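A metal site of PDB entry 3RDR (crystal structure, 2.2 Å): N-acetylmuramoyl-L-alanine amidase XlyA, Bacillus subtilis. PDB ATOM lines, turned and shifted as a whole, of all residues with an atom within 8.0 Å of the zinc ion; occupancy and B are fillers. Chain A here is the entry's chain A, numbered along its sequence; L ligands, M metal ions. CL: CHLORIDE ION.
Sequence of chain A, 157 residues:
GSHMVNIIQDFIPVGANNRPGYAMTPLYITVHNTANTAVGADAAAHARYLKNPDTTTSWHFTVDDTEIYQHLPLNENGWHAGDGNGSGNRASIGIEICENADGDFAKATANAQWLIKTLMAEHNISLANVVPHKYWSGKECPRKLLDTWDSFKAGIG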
ATOM      1  N   THR A  30      -7.038  18.125  17.850  1.00  0.00           N
ATOM      2  CA  THR A  30      -6.932  19.409  17.170  1.00  0.00           C
ATOM      3  C   THR A  30      -5.510  19.696  16.686  1.00  0.00           C
ATOM      4  O   THR A  30      -4.560  19.696  17.462  1.00  0.00           O
ATOM      5  CB  THR A  30      -7.415  20.539  18.102  1.00  0.00           C
ATOM      6  OG1 THR A  30      -8.757  20.258  18.533  1.00  0.00           O
ATOM      7  CG2 THR A  30      -7.397  21.881  17.387  1.00  0.00           C
ATOM      8  N   VAL A  31      -5.371  19.970  15.392  1.00  0.00           N
ATOM      9  CA  VAL A  31      -4.061  20.239  14.788  1.00  0.00           C
ATOM     10  C   VAL A  31      -3.757  21.715  14.571  1.00  0.00           C
ATOM     11  O   VAL A  31      -4.601  22.468  14.100  1.00  0.00           O
ATOM     12  CB  VAL A  31      -3.950  19.517  13.421  1.00  0.00           C
ATOM     13  CG1 VAL A  31      -2.565  19.741  12.815  1.00  0.00           C
ATOM     14  CG2 VAL A  31      -4.226  18.032  13.605  1.00  0.00           C
ATOM     15  N   HIS A  32      -2.529  22.098  14.917  1.00  0.00           N
ATOM     16  CA  HIS A  32      -2.054  23.478  14.774  1.00  0.00           C
ATOM     17  C   HIS A  32      -0.718  23.508  14.035  1.00  0.00           C
ATOM     18  O   HIS A  32      -0.080  22.469  13.831  1.00  0.00           O
ATOM     19  CB  HIS A  32      -1.780  24.112  16.154  1.00  0.00           C
ATOM     20  CG  HIS A  32      -2.927  24.056  17.119  1.00  0.00           C
ATOM     21  ND1 HIS A  32      -3.728  25.146  17.382  1.00  0.00           N
ATOM     22  CD2 HIS A  32      -3.351  23.072  17.945  1.00  0.00           C
ATOM     23  CE1 HIS A  32      -4.600  24.836  18.330  1.00  0.00           C
ATOM     24  NE2 HIS A  32      -4.393  23.579  18.687  1.00  0.00           N
ATOM     25  N   ASN A  33      -0.298  24.705  13.656  1.00  0.00           N
ATOM     26  CA  ASN A  33       0.997  24.947  13.011  1.00  0.00           C
ATOM     27  C   ASN A  33       1.504  26.144  13.827  1.00  0.00           C
ATOM     28  O   ASN A  33       0.774  27.107  14.004  1.00  0.00           O
ATOM     29  CB  ASN A  33       0.837  25.345  11.534  1.00  0.00           C
ATOM     30  CG  ASN A  33       0.711  24.133  10.612  1.00  0.00           C
ATOM     31  OD1 ASN A  33       0.466  24.288   9.409  1.00  0.00           O
ATOM     32  ND2 ASN A  33       0.882  22.931  11.162  1.00  0.00           N
ATOM     33  N   THR A  34       2.738  26.076  14.312  1.00  0.00           N
ATOM     34  CA  THR A  34       3.292  27.143  15.149  1.00  0.00           C
ATOM     35  C   THR A  34       3.416  28.526  14.495  1.00  0.00           C
ATOM     36  O   THR A  34       3.422  29.534  15.202  1.00  0.00           O
ATOM     37  CB  THR A  34       4.687  26.773  15.678  1.00  0.00           C
ATOM     38  OG1 THR A  34       5.597  26.651  14.579  1.00  0.00           O
ATOM     39  CG2 THR A  34       4.644  25.439  16.435  1.00  0.00           C
ATOM     40  N   THR A  57      -1.180  30.130  27.033  1.00  0.00           N
ATOM     41  CA  THR A  57      -1.641  29.128  26.071  1.00  0.00           C
ATOM     42  C   THR A  57      -0.924  27.805  26.320  1.00  0.00           C
ATOM     43  O   THR A  57       0.193  27.773  26.845  1.00  0.00           O
ATOM     44  CB  THR A  57      -1.369  29.590  24.607  1.00  0.00           C
ATOM     45  OG1 THR A  57      -2.220  30.692  24.286  1.00  0.00           O
ATOM     46  CG2 THR A  57      -1.641  28.465  23.622  1.00  0.00           C
ATOM     47  N   TRP A  59      -0.882  23.301  24.954  1.00  0.00           N
ATOM     48  CA  TRP A  59      -1.393  22.178  24.181  1.00  0.00           C
ATOM     49  C   TRP A  59      -0.627  20.946  24.637  1.00  0.00           C
ATOM     50  O   TRP A  59       0.323  21.052  25.415  1.00  0.00           O
ATOM     51  CB  TRP A  59      -1.212  22.439  22.675  1.00  0.00           C
ATOM     52  CG  TRP A  59       0.171  22.812  22.302  1.00  0.00           C
ATOM     53  CD1 TRP A  59       1.168  21.964  21.895  1.00  0.00           C
ATOM     54  CD2 TRP A  59       0.751  24.119  22.326  1.00  0.00           C
ATOM     55  NE1 TRP A  59       2.317  22.662  21.661  1.00  0.00           N
ATOM     56  CE2 TRP A  59       2.089  23.992  21.924  1.00  0.00           C
ATOM     57  CE3 TRP A  59       0.258  25.385  22.652  1.00  0.00           C
ATOM     58  CZ2 TRP A  59       2.962  25.091  21.832  1.00  0.00           C
ATOM     59  CZ3 TRP A  59       1.121  26.487  22.564  1.00  0.00           C
ATOM     60  CH2 TRP A  59       2.448  26.322  22.162  1.00  0.00           C
ATOM     61  N   HIS A  80      -6.035  26.141  23.940  1.00  0.00           N
ATOM     62  CA  HIS A  80      -5.476  26.305  22.601  1.00  0.00           C
ATOM     63  C   HIS A  80      -6.457  26.449  21.454  1.00  0.00           C
ATOM     64  O   HIS A  80      -6.102  27.003  20.411  1.00  0.00           O
ATOM     65  CB  HIS A  80      -4.558  25.116  22.314  1.00  0.00           C
ATOM     66  CG  HIS A  80      -5.257  23.794  22.366  1.00  0.00           C
ATOM     67  ND1 HIS A  80      -5.867  23.225  21.264  1.00  0.00           N
ATOM     68  CD2 HIS A  80      -5.526  22.973  23.410  1.00  0.00           C
ATOM     69  CE1 HIS A  80      -6.470  22.116  21.627  1.00  0.00           C
ATOM     70  NE2 HIS A  80      -6.282  21.938  22.925  1.00  0.00           N
ATOM     71  N   ALA A  81      -7.689  25.954  21.636  1.00  0.00           N
ATOM     72  CA  ALA A  81      -8.698  25.991  20.585  1.00  0.00           C
ATOM     73  C   ALA A  81      -9.451  27.305  20.445  1.00  0.00           C
ATOM     74  O   ALA A  81     -10.079  27.559  19.413  1.00  0.00           O
ATOM     75  CB  ALA A  81      -9.684  24.844  20.790  1.00  0.00           C
ATOM     76  N   GLY A  82      -9.417  28.148  21.478  1.00  0.00           N
ATOM     77  CA  GLY A  82     -10.086  29.425  21.431  1.00  0.00           C
ATOM     78  C   GLY A  82     -11.609  29.377  21.475  1.00  0.00           C
ATOM     79  O   GLY A  82     -12.265  30.313  21.017  1.00  0.00           O
ATOM     80  N   ILE A  95      -2.280  19.444  19.194  1.00  0.00           N
ATOM     81  CA  ILE A  95      -0.982  19.119  18.601  1.00  0.00           C
ATOM     82  C   ILE A  95      -0.447  20.279  17.774  1.00  0.00           C
ATOM     83  O   ILE A  95      -1.135  20.824  16.917  1.00  0.00           O
ATOM     84  CB  ILE A  95      -1.054  17.869  17.676  1.00  0.00           C
ATOM     85  CG1 ILE A  95      -1.461  16.628  18.466  1.00  0.00           C
ATOM     86  CG2 ILE A  95       0.320  17.615  17.051  1.00  0.00           C
ATOM     87  CD1 ILE A  95      -2.927  16.564  18.788  1.00  0.00           C
ATOM     88  N   GLU A  96       0.805  20.654  18.024  1.00  0.00           N
ATOM     89  CA  GLU A  96       1.443  21.728  17.265  1.00  0.00           C
ATOM     90  C   GLU A  96       2.519  21.126  16.381  1.00  0.00           C
ATOM     91  O   GLU A  96       3.270  20.244  16.808  1.00  0.00           O
ATOM     92  CB  GLU A  96       2.076  22.762  18.207  1.00  0.00           C
ATOM     93  CG  GLU A  96       1.116  23.818  18.732  1.00  0.00           C
ATOM     94  CD  GLU A  96       0.882  24.955  17.735  1.00  0.00           C
ATOM     95  OE1 GLU A  96       1.277  24.815  16.553  1.00  0.00           O
ATOM     96  OE2 GLU A  96       0.298  25.988  18.124  1.00  0.00           O
ATOM     97  N   PRO A 132      -8.960  20.678  12.471  1.00  0.00           N
ATOM     98  CA  PRO A 132      -8.006  21.794  12.480  1.00  0.00           C
ATOM     99  C   PRO A 132      -8.485  22.798  13.514  1.00  0.00           C
ATOM    100  O   PRO A 132      -9.676  22.857  13.808  1.00  0.00           O
ATOM    101  CB  PRO A 132      -8.114  22.345  11.065  1.00  0.00           C
ATOM    102  CG  PRO A 132      -9.584  22.163  10.771  1.00  0.00           C
ATOM    103  CD  PRO A 132      -9.855  20.773  11.297  1.00  0.00           C
ATOM    104  N   HIS A 133      -7.558  23.569  14.064  1.00  0.00           N
ATOM    105  CA  HIS A 133      -7.912  24.596  15.031  1.00  0.00           C
ATOM    106  C   HIS A 133      -9.075  25.418  14.475  1.00  0.00           C
ATOM    107  O   HIS A 133      -9.993  25.792  15.207  1.00  0.00           O
ATOM    108  CB  HIS A 133      -6.700  25.497  15.303  1.00  0.00           C
ATOM    109  CG  HIS A 133      -6.977  26.636  16.232  1.00  0.00           C
ATOM    110  ND1 HIS A 133      -6.025  27.566  16.564  1.00  0.00           N
ATOM    111  CD2 HIS A 133      -8.095  26.989  16.909  1.00  0.00           C
ATOM    112  CE1 HIS A 133      -6.545  28.446  17.406  1.00  0.00           C
ATOM    113  NE2 HIS A 133      -7.800  28.116  17.626  1.00  0.00           N
ATOM    114  N   LYS A 134      -9.018  25.686  13.180  1.00  0.00           N
ATOM    115  CA  LYS A 134     -10.043  26.485  12.514  1.00  0.00           C
ATOM    116  C   LYS A 134     -11.471  26.021  12.797  1.00  0.00           C
ATOM    117  O   LYS A 134     -12.383  26.841  12.942  1.00  0.00           O
ATOM    118  CB  LYS A 134      -9.799  26.495  10.998  1.00  0.00           C
ATOM    119  CG  LYS A 134     -10.752  27.386  10.218  1.00  0.00           C
ATOM    120  CD  LYS A 134     -10.364  27.446   8.738  1.00  0.00           C
ATOM    121  CE  LYS A 134     -11.285  28.379   7.951  1.00  0.00           C
ATOM    122  NZ  LYS A 134     -10.863  28.439   6.523  1.00  0.00           N
ATOM    123  N   SER A 137     -12.601  27.700  16.015  1.00  0.00           N
ATOM    124  CA  SER A 137     -12.589  29.153  16.113  1.00  0.00           C
ATOM    125  C   SER A 137     -12.604  29.926  14.806  1.00  0.00           C
ATOM    126  O   SER A 137     -12.689  31.147  14.819  1.00  0.00           O
ATOM    127  CB  SER A 137     -11.353  29.577  16.903  1.00  0.00           C
ATOM    128  OG  SER A 137     -10.176  29.196  16.200  1.00  0.00           O
ATOM    129  N   LYS A 139     -10.214  30.386  13.031  1.00  0.00           N
ATOM    130  CA  LYS A 139      -8.876  30.952  12.860  1.00  0.00           C
ATOM    131  C   LYS A 139      -8.162  30.210  11.733  1.00  0.00           C
ATOM    132  O   LYS A 139      -8.388  29.022  11.521  1.00  0.00           O
ATOM    133  CB  LYS A 139      -8.082  30.836  14.157  1.00  0.00           C
ATOM    134  CG  LYS A 139      -6.695  31.461  14.114  1.00  0.00           C
ATOM    135  CD  LYS A 139      -6.053  31.498  15.498  1.00  0.00           C
ATOM    136  CE  LYS A 139      -6.812  32.421  16.437  1.00  0.00           C
ATOM    137  NZ  LYS A 139      -6.234  32.447  17.813  1.00  0.00           N
ATOM    138  N   GLU A 140      -7.305  30.923  11.010  1.00  0.00           N
ATOM    139  CA  GLU A 140      -6.575  30.323   9.893  1.00  0.00           C
ATOM    140  C   GLU A 140      -5.365  29.529  10.380  1.00  0.00           C
ATOM    141  O   GLU A 140      -4.204  29.909  10.169  1.00  0.00           O
ATOM    142  CB  GLU A 140      -6.139  31.429   8.925  1.00  0.00           C
ATOM    143  CG  GLU A 140      -6.453  31.152   7.451  1.00  0.00           C
ATOM    144  CD  GLU A 140      -7.932  30.880   7.204  1.00  0.00           C
ATOM    145  OE1 GLU A 140      -8.776  31.669   7.696  1.00  0.00           O
ATOM    146  OE2 GLU A 140      -8.263  29.900   6.507  1.00  0.00           O
ATOM    147  N   CYS A 141      -5.644  28.404  11.037  1.00  0.00           N
ATOM    148  CA  CYS A 141      -4.620  27.511  11.584  1.00  0.00           C
ATOM    149  C   CYS A 141      -5.221  26.116  11.494  1.00  0.00           C
ATOM    150  O   CYS A 141      -6.396  25.929  11.796  1.00  0.00           O
ATOM    151  CB  CYS A 141      -4.337  27.880  13.049  1.00  0.00           C
ATOM    152  SG  CYS A 141      -3.197  26.753  13.912  1.00  0.00           S
ATOM    153  N   PRO A 142      -4.416  25.098  11.108  1.00  0.00           N
ATOM    154  CA  PRO A 142      -2.995  25.092  10.731  1.00  0.00           C
ATOM    155  C   PRO A 142      -2.766  25.726   9.357  1.00  0.00           C
ATOM    156  O   PRO A 142      -3.091  25.141   8.326  1.00  0.00           O
ATOM    157  CB  PRO A 142      -2.654  23.603  10.773  1.00  0.00           C
ATOM    158  CG  PRO A 142      -3.911  22.977  10.269  1.00  0.00           C
ATOM    159  CD  PRO A 142      -5.008  23.752  10.976  1.00  0.00           C
ATOM    160  N   ARG A 143      -2.178  26.915   9.354  1.00  0.00           N
ATOM    161  CA  ARG A 143      -1.943  27.673   8.143  1.00  0.00           C
ATOM    162  C   ARG A 143      -1.302  26.954   6.960  1.00  0.00           C
ATOM    163  O   ARG A 143      -1.607  27.274   5.811  1.00  0.00           O
ATOM    164  CB  ARG A 143      -1.146  28.945   8.467  1.00  0.00           C
ATOM    165  CG  ARG A 143       0.306  28.714   8.893  1.00  0.00           C
ATOM    166  CD  ARG A 143       1.016  30.044   9.075  1.00  0.00           C
ATOM    167  NE  ARG A 143       2.467  29.894   9.090  1.00  0.00           N
ATOM    168  CZ  ARG A 143       3.335  30.912   9.131  1.00  0.00           C
ATOM    169  NH1 ARG A 143       2.882  32.164   9.159  1.00  0.00           N
ATOM    170  NH2 ARG A 143       4.629  30.676   9.132  1.00  0.00           N
HETATM  171 CL    CL L   1      -2.890  28.833  17.290  1.00  0.00          CL
HETATM  172 ZN    ZN M   1      -3.869  27.028  16.209  1.00  0.00          ZN
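NE2 of His 32 is in hydrogen-bond range of ND1 of His 80, 3.0 Å away.
The backbone NH (N) of His 32 is in hydrogen-bond range of the backbone carbonyl oxygen (O) of Ile 95.
The backbone carbonyl oxygen of His 80 lies close to a ring nitrogen (NE2) of His 133 (3.4 Å).
N of His 133 sits at hydrogen-bond distance from O of Val 31 (3.2 Å).
A ring nitrogen (NE2) of His 133 lies within hydrogen-bond range of the backbone carbonyl oxygen (O) of Ala 81, at 2.9 Å.
The side-chain hydroxyl of Ser 137 lies within hydrogen-bond range of a ring nitrogen (NE2) of His 133 (3.0 Å).
SG of Cys 141 lies close to N of Asn 33, 3.6 Å away.
O of Cys 141 lies within hydrogen-bond range of N of Lys 134 (3.0 Å).
Of the 21 residues printed, 3 come within 4 Å of the zinc ion.
Along chain A the residues within 4 Å of the zinc ion span positions 32 to 141.
A ring nitrogen (ND1) of His 32 binds the zinc ion (2.2 Å).
ND1 of His 133 is bound to the zinc ion (2.3 Å).
The zinc ion is bound by a chlorine (CL) of the ligand (2.3 Å).
SG of Cys 141 binds the zinc ion (2.4 Å).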
